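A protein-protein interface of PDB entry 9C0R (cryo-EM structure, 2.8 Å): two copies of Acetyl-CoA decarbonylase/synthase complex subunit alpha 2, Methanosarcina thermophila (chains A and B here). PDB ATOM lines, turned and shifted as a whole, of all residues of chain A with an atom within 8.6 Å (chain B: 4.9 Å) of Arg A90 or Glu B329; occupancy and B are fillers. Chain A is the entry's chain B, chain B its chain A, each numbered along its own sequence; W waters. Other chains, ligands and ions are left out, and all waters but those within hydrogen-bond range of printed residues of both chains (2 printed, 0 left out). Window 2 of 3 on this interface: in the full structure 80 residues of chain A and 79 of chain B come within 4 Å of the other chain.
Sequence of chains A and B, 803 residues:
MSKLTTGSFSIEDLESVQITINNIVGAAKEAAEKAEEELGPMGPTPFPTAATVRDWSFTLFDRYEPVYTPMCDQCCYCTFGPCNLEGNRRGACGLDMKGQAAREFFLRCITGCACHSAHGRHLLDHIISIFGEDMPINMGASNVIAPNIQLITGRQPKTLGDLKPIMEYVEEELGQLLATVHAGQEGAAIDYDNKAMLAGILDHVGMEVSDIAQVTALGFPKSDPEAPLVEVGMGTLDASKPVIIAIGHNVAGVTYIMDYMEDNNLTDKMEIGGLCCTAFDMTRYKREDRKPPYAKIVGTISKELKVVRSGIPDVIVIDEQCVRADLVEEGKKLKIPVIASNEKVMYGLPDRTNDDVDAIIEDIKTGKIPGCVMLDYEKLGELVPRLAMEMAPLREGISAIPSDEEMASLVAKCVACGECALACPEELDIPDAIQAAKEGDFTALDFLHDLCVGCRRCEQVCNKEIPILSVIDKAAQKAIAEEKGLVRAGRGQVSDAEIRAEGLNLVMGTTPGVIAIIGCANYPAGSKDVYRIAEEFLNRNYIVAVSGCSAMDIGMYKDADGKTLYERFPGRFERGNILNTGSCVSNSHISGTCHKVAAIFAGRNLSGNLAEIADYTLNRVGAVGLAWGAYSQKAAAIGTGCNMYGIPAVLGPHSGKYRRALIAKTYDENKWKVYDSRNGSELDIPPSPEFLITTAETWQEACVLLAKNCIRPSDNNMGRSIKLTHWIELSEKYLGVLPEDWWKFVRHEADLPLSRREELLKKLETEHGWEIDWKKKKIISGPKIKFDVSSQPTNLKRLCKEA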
ATOM      1  N   CYS A  75      -2.953 -26.962  23.261  1.00  0.00           N
ATOM      2  CA  CYS A  75      -1.699 -26.267  23.501  1.00  0.00           C
ATOM      3  C   CYS A  75      -1.522 -26.079  24.998  1.00  0.00           C
ATOM      4  O   CYS A  75      -2.494 -25.864  25.727  1.00  0.00           O
ATOM      5  CB  CYS A  75      -1.646 -24.911  22.795  1.00  0.00           C
ATOM      6  SG  CYS A  75      -0.248 -23.874  23.298  1.00  0.00           S
ATOM      7  N   CYS A  83      -5.456 -25.175  26.209  1.00  0.00           N
ATOM      8  CA  CYS A  83      -6.506 -24.678  25.331  1.00  0.00           C
ATOM      9  C   CYS A  83      -6.853 -25.745  24.306  1.00  0.00           C
ATOM     10  O   CYS A  83      -5.973 -26.227  23.587  1.00  0.00           O
ATOM     11  CB  CYS A  83      -6.067 -23.394  24.624  1.00  0.00           C
ATOM     12  SG  CYS A  83      -5.670 -22.012  25.712  1.00  0.00           S
ATOM     13  N   ASN A  84      -8.129 -26.103  24.235  1.00  0.00           N
ATOM     14  CA  ASN A  84      -8.593 -27.069  23.248  1.00  0.00           C
ATOM     15  C   ASN A  84      -8.683 -26.388  21.889  1.00  0.00           C
ATOM     16  O   ASN A  84      -9.438 -25.426  21.720  1.00  0.00           O
ATOM     17  CB  ASN A  84      -9.944 -27.646  23.666  1.00  0.00           C
ATOM     18  CG  ASN A  84     -10.371 -28.816  22.807  1.00  0.00           C
ATOM     19  OD1 ASN A  84      -9.655 -29.228  21.898  1.00  0.00           O
ATOM     20  ND2 ASN A  84     -11.542 -29.363  23.097  1.00  0.00           N
ATOM     21  N   LEU A  85      -7.908 -26.880  20.923  1.00  0.00           N
ATOM     22  CA  LEU A  85      -7.843 -26.285  19.593  1.00  0.00           C
ATOM     23  C   LEU A  85      -8.429 -27.192  18.518  1.00  0.00           C
ATOM     24  O   LEU A  85      -8.146 -26.999  17.334  1.00  0.00           O
ATOM     25  CB  LEU A  85      -6.400 -25.926  19.242  1.00  0.00           C
ATOM     26  CG  LEU A  85      -5.568 -25.216  20.308  1.00  0.00           C
ATOM     27  CD1 LEU A  85      -4.093 -25.300  19.964  1.00  0.00           C
ATOM     28  CD2 LEU A  85      -5.998 -23.772  20.446  1.00  0.00           C
ATOM     29  N   GLU A  86      -9.237 -28.177  18.905  1.00  0.00           N
ATOM     30  CA  GLU A  86      -9.813 -29.093  17.932  1.00  0.00           C
ATOM     31  C   GLU A  86     -10.721 -28.347  16.963  1.00  0.00           C
ATOM     32  O   GLU A  86     -11.516 -27.495  17.361  1.00  0.00           O
ATOM     33  CB  GLU A  86     -10.597 -30.196  18.642  1.00  0.00           C
ATOM     34  CG  GLU A  86     -10.819 -31.432  17.797  1.00  0.00           C
ATOM     35  CD  GLU A  86     -12.107 -31.371  17.004  1.00  0.00           C
ATOM     36  OE1 GLU A  86     -13.143 -30.973  17.579  1.00  0.00           O
ATOM     37  OE2 GLU A  86     -12.087 -31.720  15.804  1.00  0.00           O
ATOM     38  N   GLY A  87     -10.598 -28.679  15.680  1.00  0.00           N
ATOM     39  CA  GLY A  87     -11.353 -27.987  14.656  1.00  0.00           C
ATOM     40  C   GLY A  87     -10.745 -26.682  14.204  1.00  0.00           C
ATOM     41  O   GLY A  87     -11.463 -25.818  13.694  1.00  0.00           O
ATOM     42  N   ASN A  88      -9.433 -26.516  14.379  1.00  0.00           N
ATOM     43  CA  ASN A  88      -8.727 -25.273  14.066  1.00  0.00           C
ATOM     44  C   ASN A  88      -9.279 -24.093  14.865  1.00  0.00           C
ATOM     45  O   ASN A  88      -9.305 -22.958  14.384  1.00  0.00           O
ATOM     46  CB  ASN A  88      -8.756 -24.970  12.563  1.00  0.00           C
ATOM     47  CG  ASN A  88      -7.658 -24.015  12.141  1.00  0.00           C
ATOM     48  OD1 ASN A  88      -6.722 -23.762  12.893  1.00  0.00           O
ATOM     49  ND2 ASN A  88      -7.770 -23.476  10.936  1.00  0.00           N
ATOM     50  N   ARG A  89      -9.723 -24.353  16.090  1.00  0.00           N
ATOM     51  CA  ARG A  89     -10.134 -23.283  16.983  1.00  0.00           C
ATOM     52  C   ARG A  89      -8.909 -22.523  17.489  1.00  0.00           C
ATOM     53  O   ARG A  89      -7.762 -22.922  17.278  1.00  0.00           O
ATOM     54  CB  ARG A  89     -10.939 -23.840  18.155  1.00  0.00           C
ATOM     55  CG  ARG A  89     -12.311 -24.348  17.767  1.00  0.00           C
ATOM     56  CD  ARG A  89     -13.280 -24.264  18.928  1.00  0.00           C
ATOM     57  NE  ARG A  89     -13.501 -25.561  19.557  1.00  0.00           N
ATOM     58  CZ  ARG A  89     -12.820 -26.015  20.599  1.00  0.00           C
ATOM     59  NH1 ARG A  89     -11.855 -25.304  21.155  1.00  0.00           N
ATOM     60  NH2 ARG A  89     -13.118 -27.211  21.098  1.00  0.00           N
ATOM     61  N   ARG A  90      -9.163 -21.411  18.167  1.00  0.00           N
ATOM     62  CA  ARG A  90      -8.103 -20.549  18.662  1.00  0.00           C
ATOM     63  C   ARG A  90      -8.002 -20.641  20.178  1.00  0.00           C
ATOM     64  O   ARG A  90      -8.994 -20.873  20.874  1.00  0.00           O
ATOM     65  CB  ARG A  90      -8.332 -19.097  18.235  1.00  0.00           C
ATOM     66  CG  ARG A  90      -8.112 -18.862  16.752  1.00  0.00           C
ATOM     67  CD  ARG A  90      -8.426 -17.437  16.355  1.00  0.00           C
ATOM     68  NE  ARG A  90      -8.309 -17.241  14.915  1.00  0.00           N
ATOM     69  CZ  ARG A  90      -7.184 -16.915  14.294  1.00  0.00           C
ATOM     70  NH1 ARG A  90      -6.055 -16.736  14.956  1.00  0.00           N
ATOM     71  NH2 ARG A  90      -7.195 -16.762  12.974  1.00  0.00           N
ATOM     72  N   GLY A  91      -6.781 -20.467  20.679  1.00  0.00           N
ATOM     73  CA  GLY A  91      -6.532 -20.479  22.102  1.00  0.00           C
ATOM     74  C   GLY A  91      -6.864 -19.152  22.747  1.00  0.00           C
ATOM     75  O   GLY A  91      -7.394 -18.232  22.126  1.00  0.00           O
ATOM     76  N   ALA A  92      -6.545 -19.058  24.038  1.00  0.00           N
ATOM     77  CA  ALA A  92      -6.821 -17.832  24.774  1.00  0.00           C
ATOM     78  C   ALA A  92      -5.986 -16.661  24.278  1.00  0.00           C
ATOM     79  O   ALA A  92      -6.385 -15.509  24.470  1.00  0.00           O
ATOM     80  CB  ALA A  92      -6.590 -18.049  26.270  1.00  0.00           C
ATOM     81  N   CYS A  93      -4.846 -16.924  23.642  1.00  0.00           N
ATOM     82  CA  CYS A  93      -4.021 -15.870  23.072  1.00  0.00           C
ATOM     83  C   CYS A  93      -4.396 -15.531  21.637  1.00  0.00           C
ATOM     84  O   CYS A  93      -3.850 -14.574  21.082  1.00  0.00           O
ATOM     85  CB  CYS A  93      -2.541 -16.264  23.123  1.00  0.00           C
ATOM     86  SG  CYS A  93      -2.134 -17.781  22.234  1.00  0.00           S
ATOM     87  N   GLY A  94      -5.308 -16.286  21.029  1.00  0.00           N
ATOM     88  CA  GLY A  94      -5.705 -16.067  19.657  1.00  0.00           C
ATOM     89  C   GLY A  94      -5.023 -16.948  18.636  1.00  0.00           C
ATOM     90  O   GLY A  94      -5.378 -16.879  17.455  1.00  0.00           O
ATOM     91  N   LEU A  95      -4.056 -17.764  19.045  1.00  0.00           N
ATOM     92  CA  LEU A  95      -3.376 -18.665  18.126  1.00  0.00           C
ATOM     93  C   LEU A  95      -4.229 -19.896  17.850  1.00  0.00           C
ATOM     94  O   LEU A  95      -4.873 -20.437  18.752  1.00  0.00           O
ATOM     95  CB  LEU A  95      -2.020 -19.083  18.695  1.00  0.00           C
ATOM     96  CG  LEU A  95      -1.073 -19.810  17.742  1.00  0.00           C
ATOM     97  CD1 LEU A  95      -0.442 -18.834  16.769  1.00  0.00           C
ATOM     98  CD2 LEU A  95      -0.009 -20.552  18.518  1.00  0.00           C
ATOM     99  N   ASP A  96      -4.222 -20.343  16.598  1.00  0.00           N
ATOM    100  CA  ASP A  96      -5.060 -21.441  16.148  1.00  0.00           C
ATOM    101  C   ASP A  96      -4.253 -22.737  16.062  1.00  0.00           C
ATOM    102  O   ASP A  96      -3.081 -22.796  16.448  1.00  0.00           O
ATOM    103  CB  ASP A  96      -5.700 -21.084  14.806  1.00  0.00           C
ATOM    104  CG  ASP A  96      -4.673 -20.838  13.722  1.00  0.00           C
ATOM    105  OD1 ASP A  96      -3.463 -20.870  14.032  1.00  0.00           O
ATOM    106  OD2 ASP A  96      -5.075 -20.611  12.561  1.00  0.00           O
ATOM    107  N   MET A  97      -4.892 -23.793  15.553  1.00  0.00           N
ATOM    108  CA  MET A  97      -4.246 -25.100  15.459  1.00  0.00           C
ATOM    109  C   MET A  97      -3.068 -25.076  14.493  1.00  0.00           C
ATOM    110  O   MET A  97      -1.997 -25.621  14.788  1.00  0.00           O
ATOM    111  CB  MET A  97      -5.261 -26.155  15.027  1.00  0.00           C
ATOM    112  CG  MET A  97      -5.069 -27.500  15.691  1.00  0.00           C
ATOM    113  SD  MET A  97      -6.371 -28.670  15.286  1.00  0.00           S
ATOM    114  CE  MET A  97      -6.123 -29.883  16.575  1.00  0.00           C
ATOM    115  N   LYS A  98      -3.255 -24.467  13.320  1.00  0.00           N
ATOM    116  CA  LYS A  98      -2.178 -24.408  12.339  1.00  0.00           C
ATOM    117  C   LYS A  98      -0.981 -23.645  12.885  1.00  0.00           C
ATOM    118  O   LYS A  98       0.169 -24.080  12.732  1.00  0.00           O
ATOM    119  CB  LYS A  98      -2.683 -23.764  11.049  1.00  0.00           C
ATOM    120  CG  LYS A  98      -3.709 -24.596  10.312  1.00  0.00           C
ATOM    121  CD  LYS A  98      -4.218 -23.890   9.073  1.00  0.00           C
ATOM    122  CE  LYS A  98      -5.225 -24.756   8.334  1.00  0.00           C
ATOM    123  NZ  LYS A  98      -5.803 -24.067   7.149  1.00  0.00           N
ATOM    124  N   GLY A  99      -1.234 -22.513  13.544  1.00  0.00           N
ATOM    125  CA  GLY A  99      -0.149 -21.758  14.142  1.00  0.00           C
ATOM    126  C   GLY A  99       0.578 -22.534  15.222  1.00  0.00           C
ATOM    127  O   GLY A  99       1.804 -22.484  15.314  1.00  0.00           O
ATOM    128  N   GLN A 100      -0.169 -23.270  16.049  1.00  0.00           N
ATOM    129  CA  GLN A 100       0.460 -24.042  17.116  1.00  0.00           C
ATOM    130  C   GLN A 100       1.308 -25.180  16.557  1.00  0.00           C
ATOM    131  O   GLN A 100       2.407 -25.441  17.057  1.00  0.00           O
ATOM    132  CB  GLN A 100      -0.601 -24.575  18.079  1.00  0.00           C
ATOM    133  CG  GLN A 100      -0.086 -25.595  19.088  1.00  0.00           C
ATOM    134  CD  GLN A 100       0.915 -25.018  20.077  1.00  0.00           C
ATOM    135  OE1 GLN A 100       1.099 -23.807  20.163  1.00  0.00           O
ATOM    136  NE2 GLN A 100       1.566 -25.893  20.829  1.00  0.00           N
ATOM    137  N   GLU A 186       4.028 -14.587  17.826  1.00  0.00           N
ATOM    138  CA  GLU A 186       3.785 -14.719  16.398  1.00  0.00           C
ATOM    139  C   GLU A 186       2.409 -15.334  16.208  1.00  0.00           C
ATOM    140  O   GLU A 186       2.052 -16.291  16.901  1.00  0.00           O
ATOM    141  CB  GLU A 186       4.858 -15.574  15.714  1.00  0.00           C
ATOM    142  CG  GLU A 186       4.634 -15.786  14.226  1.00  0.00           C
ATOM    143  CD  GLU A 186       4.782 -14.507  13.425  1.00  0.00           C
ATOM    144  OE1 GLU A 186       5.928 -14.050  13.236  1.00  0.00           O
ATOM    145  OE2 GLU A 186       3.753 -13.960  12.986  1.00  0.00           O
ATOM    146  N   GLY A 187       1.643 -14.782  15.274  1.00  0.00           N
ATOM    147  CA  GLY A 187       0.273 -15.215  15.097  1.00  0.00           C
ATOM    148  C   GLY A 187       0.026 -16.048  13.859  1.00  0.00           C
ATOM    149  O   GLY A 187      -0.951 -16.799  13.798  1.00  0.00           O
ATOM    150  N   ALA A 188       0.898 -15.928  12.867  1.00  0.00           N
ATOM    151  CA  ALA A 188       0.728 -16.607  11.592  1.00  0.00           C
ATOM    152  C   ALA A 188       1.645 -17.818  11.510  1.00  0.00           C
ATOM    153  O   ALA A 188       2.779 -17.790  11.997  1.00  0.00           O
ATOM    154  CB  ALA A 188       1.008 -15.657  10.429  1.00  0.00           C
ATOM    155  N   ALA A 189       1.141 -18.889  10.894  1.00  0.00           N
ATOM    156  CA  ALA A 189       1.927 -20.105  10.738  1.00  0.00           C
ATOM    157  C   ALA A 189       2.997 -19.971   9.660  1.00  0.00           C
ATOM    158  O   ALA A 189       4.053 -20.605   9.761  1.00  0.00           O
ATOM    159  CB  ALA A 189       1.003 -21.282  10.424  1.00  0.00           C
ATOM    160  N   ALA B 325      -2.841 -13.030  18.837  1.00  0.00           N
ATOM    161  CA  ALA B 325      -2.679 -13.560  17.491  1.00  0.00           C
ATOM    162  C   ALA B 325      -3.894 -13.338  16.602  1.00  0.00           C
ATOM    163  O   ALA B 325      -3.810 -13.591  15.396  1.00  0.00           O
ATOM    164  CB  ALA B 325      -2.359 -15.054  17.547  1.00  0.00           C
ATOM    165  N   ASP B 326      -5.012 -12.870  17.151  1.00  0.00           N
ATOM    166  CA  ASP B 326      -6.216 -12.621  16.370  1.00  0.00           C
ATOM    167  C   ASP B 326      -6.502 -11.130  16.222  1.00  0.00           C
ATOM    168  O   ASP B 326      -7.650 -10.730  16.018  1.00  0.00           O
ATOM    169  CB  ASP B 326      -7.416 -13.337  16.990  1.00  0.00           C
ATOM    170  CG  ASP B 326      -7.712 -12.867  18.397  1.00  0.00           C
ATOM    171  OD1 ASP B 326      -6.941 -12.039  18.923  1.00  0.00           O
ATOM    172  OD2 ASP B 326      -8.718 -13.326  18.979  1.00  0.00           O
ATOM    173  N   LEU B 327      -5.465 -10.296  16.326  1.00  0.00           N
ATOM    174  CA  LEU B 327      -5.663  -8.856  16.193  1.00  0.00           C
ATOM    175  C   LEU B 327      -6.119  -8.481  14.790  1.00  0.00           C
ATOM    176  O   LEU B 327      -6.992  -7.624  14.627  1.00  0.00           O
ATOM    177  CB  LEU B 327      -4.381  -8.108  16.554  1.00  0.00           C
ATOM    178  CG  LEU B 327      -4.024  -8.020  18.036  1.00  0.00           C
ATOM    179  CD1 LEU B 327      -3.040  -6.892  18.262  1.00  0.00           C
ATOM    180  CD2 LEU B 327      -5.270  -7.828  18.885  1.00  0.00           C
ATOM    181  N   VAL B 328      -5.541  -9.106  13.763  1.00  0.00           N
ATOM    182  CA  VAL B 328      -5.907  -8.762  12.393  1.00  0.00           C
ATOM    183  C   VAL B 328      -7.320  -9.241  12.077  1.00  0.00           C
ATOM    184  O   VAL B 328      -8.112  -8.515  11.466  1.00  0.00           O
ATOM    185  CB  VAL B 328      -4.871  -9.328  11.404  1.00  0.00           C
ATOM    186  CG1 VAL B 328      -5.532  -9.715  10.088  1.00  0.00           C
ATOM    187  CG2 VAL B 328      -3.768  -8.316  11.164  1.00  0.00           C
ATOM    188  N   GLU B 329      -7.633 -10.476  12.466  1.00  0.00           N
ATOM    189  CA  GLU B 329      -8.990 -10.997  12.214  1.00  0.00           C
ATOM    190  C   GLU B 329     -10.120 -10.202  12.919  1.00  0.00           C
ATOM    191  O   GLU B 329     -11.174  -9.799  12.327  1.00  0.00           O
ATOM    192  CB  GLU B 329      -9.070 -12.459  12.653  1.00  0.00           C
ATOM    193  CG  GLU B 329      -7.991 -13.355  12.063  1.00  0.00           C
ATOM    194  CD  GLU B 329      -8.284 -13.766  10.631  1.00  0.00           C
ATOM    195  OE1 GLU B 329      -8.303 -12.885   9.746  1.00  0.00           O
ATOM    196  OE2 GLU B 329      -8.494 -14.973  10.389  1.00  0.00           O
ATOM    197  N   GLU B 330      -9.854  -9.820  14.167  1.00  0.00           N
ATOM    198  CA  GLU B 330     -10.833  -9.035  14.905  1.00  0.00           C
ATOM    199  C   GLU B 330     -10.812  -7.561  14.528  1.00  0.00           C
ATOM    200  O   GLU B 330     -11.795  -6.857  14.784  1.00  0.00           O
ATOM    201  CB  GLU B 330     -10.600  -9.186  16.409  1.00  0.00           C
ATOM    202  CG  GLU B 330     -11.156 -10.474  16.993  1.00  0.00           C
ATOM    203  CD  GLU B 330     -12.639 -10.386  17.285  1.00  0.00           C
ATOM    204  OE1 GLU B 330     -13.177  -9.259  17.305  1.00  0.00           O
ATOM    205  OE2 GLU B 330     -13.269 -11.443  17.492  1.00  0.00           O
ATOM    206  N   GLY B 331      -9.727  -7.081  13.927  1.00  0.00           N
ATOM    207  CA  GLY B 331      -9.622  -5.690  13.544  1.00  0.00           C
ATOM    208  C   GLY B 331     -10.144  -5.400  12.155  1.00  0.00           C
ATOM    209  O   GLY B 331     -10.612  -4.291  11.888  1.00  0.00           O
ATOM    210  N   LYS B 332     -10.076  -6.387  11.257  1.00  0.00           N
ATOM    211  CA  LYS B 332     -10.585  -6.184   9.905  1.00  0.00           C
ATOM    212  C   LYS B 332     -12.103  -6.095   9.873  1.00  0.00           C
ATOM    213  O   LYS B 332     -12.658  -5.555   8.911  1.00  0.00           O
ATOM    214  CB  LYS B 332     -10.104  -7.302   8.980  1.00  0.00           C
ATOM    215  CG  LYS B 332     -11.003  -8.526   8.954  1.00  0.00           C
ATOM    216  CD  LYS B 332     -10.581  -9.499   7.865  1.00  0.00           C
ATOM    217  CE  LYS B 332      -9.122  -9.889   8.002  1.00  0.00           C
ATOM    218  NZ  LYS B 332      -8.911 -11.329   7.697  1.00  0.00           N
ATOM    219  N   LYS B 333     -12.784  -6.616  10.894  1.00  0.00           N
ATOM    220  CA  LYS B 333     -14.226  -6.423  10.993  1.00  0.00           C
ATOM    221  C   LYS B 333     -14.560  -4.970  11.296  1.00  0.00           C
ATOM    222  O   LYS B 333     -15.556  -4.435  10.796  1.00  0.00           O
ATOM    223  CB  LYS B 333     -14.806  -7.342  12.069  1.00  0.00           C
ATOM    224  CG  LYS B 333     -14.490  -8.814  11.870  1.00  0.00           C
ATOM    225  CD  LYS B 333     -15.414  -9.686  12.702  1.00  0.00           C
ATOM    226  CE  LYS B 333     -14.746 -10.994  13.085  1.00  0.00           C
ATOM    227  NZ  LYS B 333     -13.792 -11.459  12.041  1.00  0.00           N
ATOM    228  N   ARG B 457     -12.541 -17.401  24.378  1.00  0.00           N
ATOM    229  CA  ARG B 457     -12.588 -18.853  24.245  1.00  0.00           C
ATOM    230  C   ARG B 457     -14.000 -19.394  24.421  1.00  0.00           C
ATOM    231  O   ARG B 457     -14.276 -20.520  23.998  1.00  0.00           O
ATOM    232  CB  ARG B 457     -11.643 -19.517  25.247  1.00  0.00           C
ATOM    233  CG  ARG B 457     -10.421 -20.158  24.607  1.00  0.00           C
ATOM    234  CD  ARG B 457      -9.352 -20.524  25.627  1.00  0.00           C
ATOM    235  NE  ARG B 457      -9.885 -21.263  26.764  1.00  0.00           N
ATOM    236  CZ  ARG B 457      -9.142 -21.849  27.693  1.00  0.00           C
ATOM    237  NH1 ARG B 457      -7.821 -21.816  27.643  1.00  0.00           N
ATOM    238  NH2 ARG B 457      -9.738 -22.481  28.699  1.00  0.00           N
ATOM    239  N   GLN B 460     -16.198 -19.487  20.787  1.00  0.00           N
ATOM    240  CA  GLN B 460     -15.944 -20.503  19.774  1.00  0.00           C
ATOM    241  C   GLN B 460     -16.615 -21.837  20.073  1.00  0.00           C
ATOM    242  O   GLN B 460     -16.525 -22.750  19.248  1.00  0.00           O
ATOM    243  CB  GLN B 460     -14.437 -20.703  19.610  1.00  0.00           C
ATOM    244  CG  GLN B 460     -13.696 -19.428  19.260  1.00  0.00           C
ATOM    245  CD  GLN B 460     -12.194 -19.592  19.297  1.00  0.00           C
ATOM    246  OE1 GLN B 460     -11.587 -20.041  18.327  1.00  0.00           O
ATOM    247  NE2 GLN B 460     -11.583 -19.220  20.416  1.00  0.00           N
HETATM  248  O   HOH W   1     -16.620 -25.902  18.946  1.00  0.00           O
HETATM  249  O   HOH W   2      -9.924 -17.365  21.642  1.00  0.00           O
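Water W2 bridges the backbone carbonyl oxygen (O) of Gly A91 and the side-chain amide nitrogen (NE2) of Gln B460. Water W1 bridges O of Gln B460 and NE of Arg A89.
Among the printed residues, merely in contact across the chains: Gly A94 with Ala B325 (3.4 Å), Leu A95 with Ala B325 (3.5 Å), Ala A92 with Arg B457 (3.5 Å), Arg A89 with Gln B460 (3.6 Å), Gly A187 with Ala B325 (3.6 Å), Arg A90 with Ala B325 (3.9 Å) and Gly A94 with Asp B326 (3.98 Å).
N of Ala B325 sits at hydrogen-bond distance from O of Cys A93. The guanidinium group of Arg A90 is in salt-bridge range of the side-chain carboxylate of Glu B329 (3.4 Å). NH1 of Arg B457 sits close to SG of Cys A83 (2.9 Å). OE1 of Gln B460 is in hydrogen-bond range of N of Arg A90, at 2.8 Å.
Printed residues of chain B within 4 Å of Arg A90: Ala B325, Glu B329 and Gln B460. Of the printed residues of chain A, Glu B329 touches Arg A90. Printed residues of chain B within 4 Å of Ala A92: Arg B457. Printed residues of chain A within 4 Å of Ala B325: Arg A90, Cys A93, Gly A94, Leu A95 and Gly A187. Printed residues of chain A within 4 Å of Asp B326: Gly A94 (3.98 Å). Of the printed residues of chain B, Arg A89 touches Gln B460 (3.6 Å). Printed residues of chain A within 4 Å of Arg B457: Cys A83 and Ala A92. Glu A86 touches none of the printed residues of chain B. Val B328 touches none of the printed residues of chain A. The nearest printed residue of chain B that does not touch Arg A90 is Arg B457 (4.1 Å). The nearest printed residue of chain A that does not touch Glu B329 is Asp A96 (6.9 Å).
Of the 23 printed residues of chain A, 8 touch a printed residue of chain B. Hydrophobic or aromatic side chains of chain A that line the printed part of chain B: Ala A92. Printed residues of chain B that touch a printed residue of chain A: Ala B325, Asp B326, Glu B329, Arg B457 and Gln B460. Hydrophobic or aromatic side chains of chain B that line the printed part of chain A: Ala B325. Among the printed residues, Asp or Glu carboxylates within 4 Å of a Lys or Arg side-chain nitrogen of the other chain: Arg A90 with Glu B329.
No position is printed for both chains. Of the 11 pairs that touch across the chains among the printed residues, none has its exchanged pair printed and touching as well.
The side-chain amino group of Lys B332 lies within salt-bridge range of the side-chain carboxylate of Glu B329 (2.6 Å). The side-chain amino group (NZ) of Lys B333 is in hydrogen-bond range of the backbone carbonyl oxygen (O) of Glu B329 (3.1 Å). The backbone carbonyl oxygen (O) of Cys A75 is in hydrogen-bond range of the backbone NH (N) of Cys A83, at 3.1 Å. The backbone NH (N) of Ala A92 lies close to the side-chain sulfur (SG) of Cys A83, at 3.5 Å. O of Asn A84 lies within hydrogen-bond range of NH1 of Arg A89 (2.5 Å). SG of Cys A93 sits close to N of Leu A95, at 3.7 Å.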
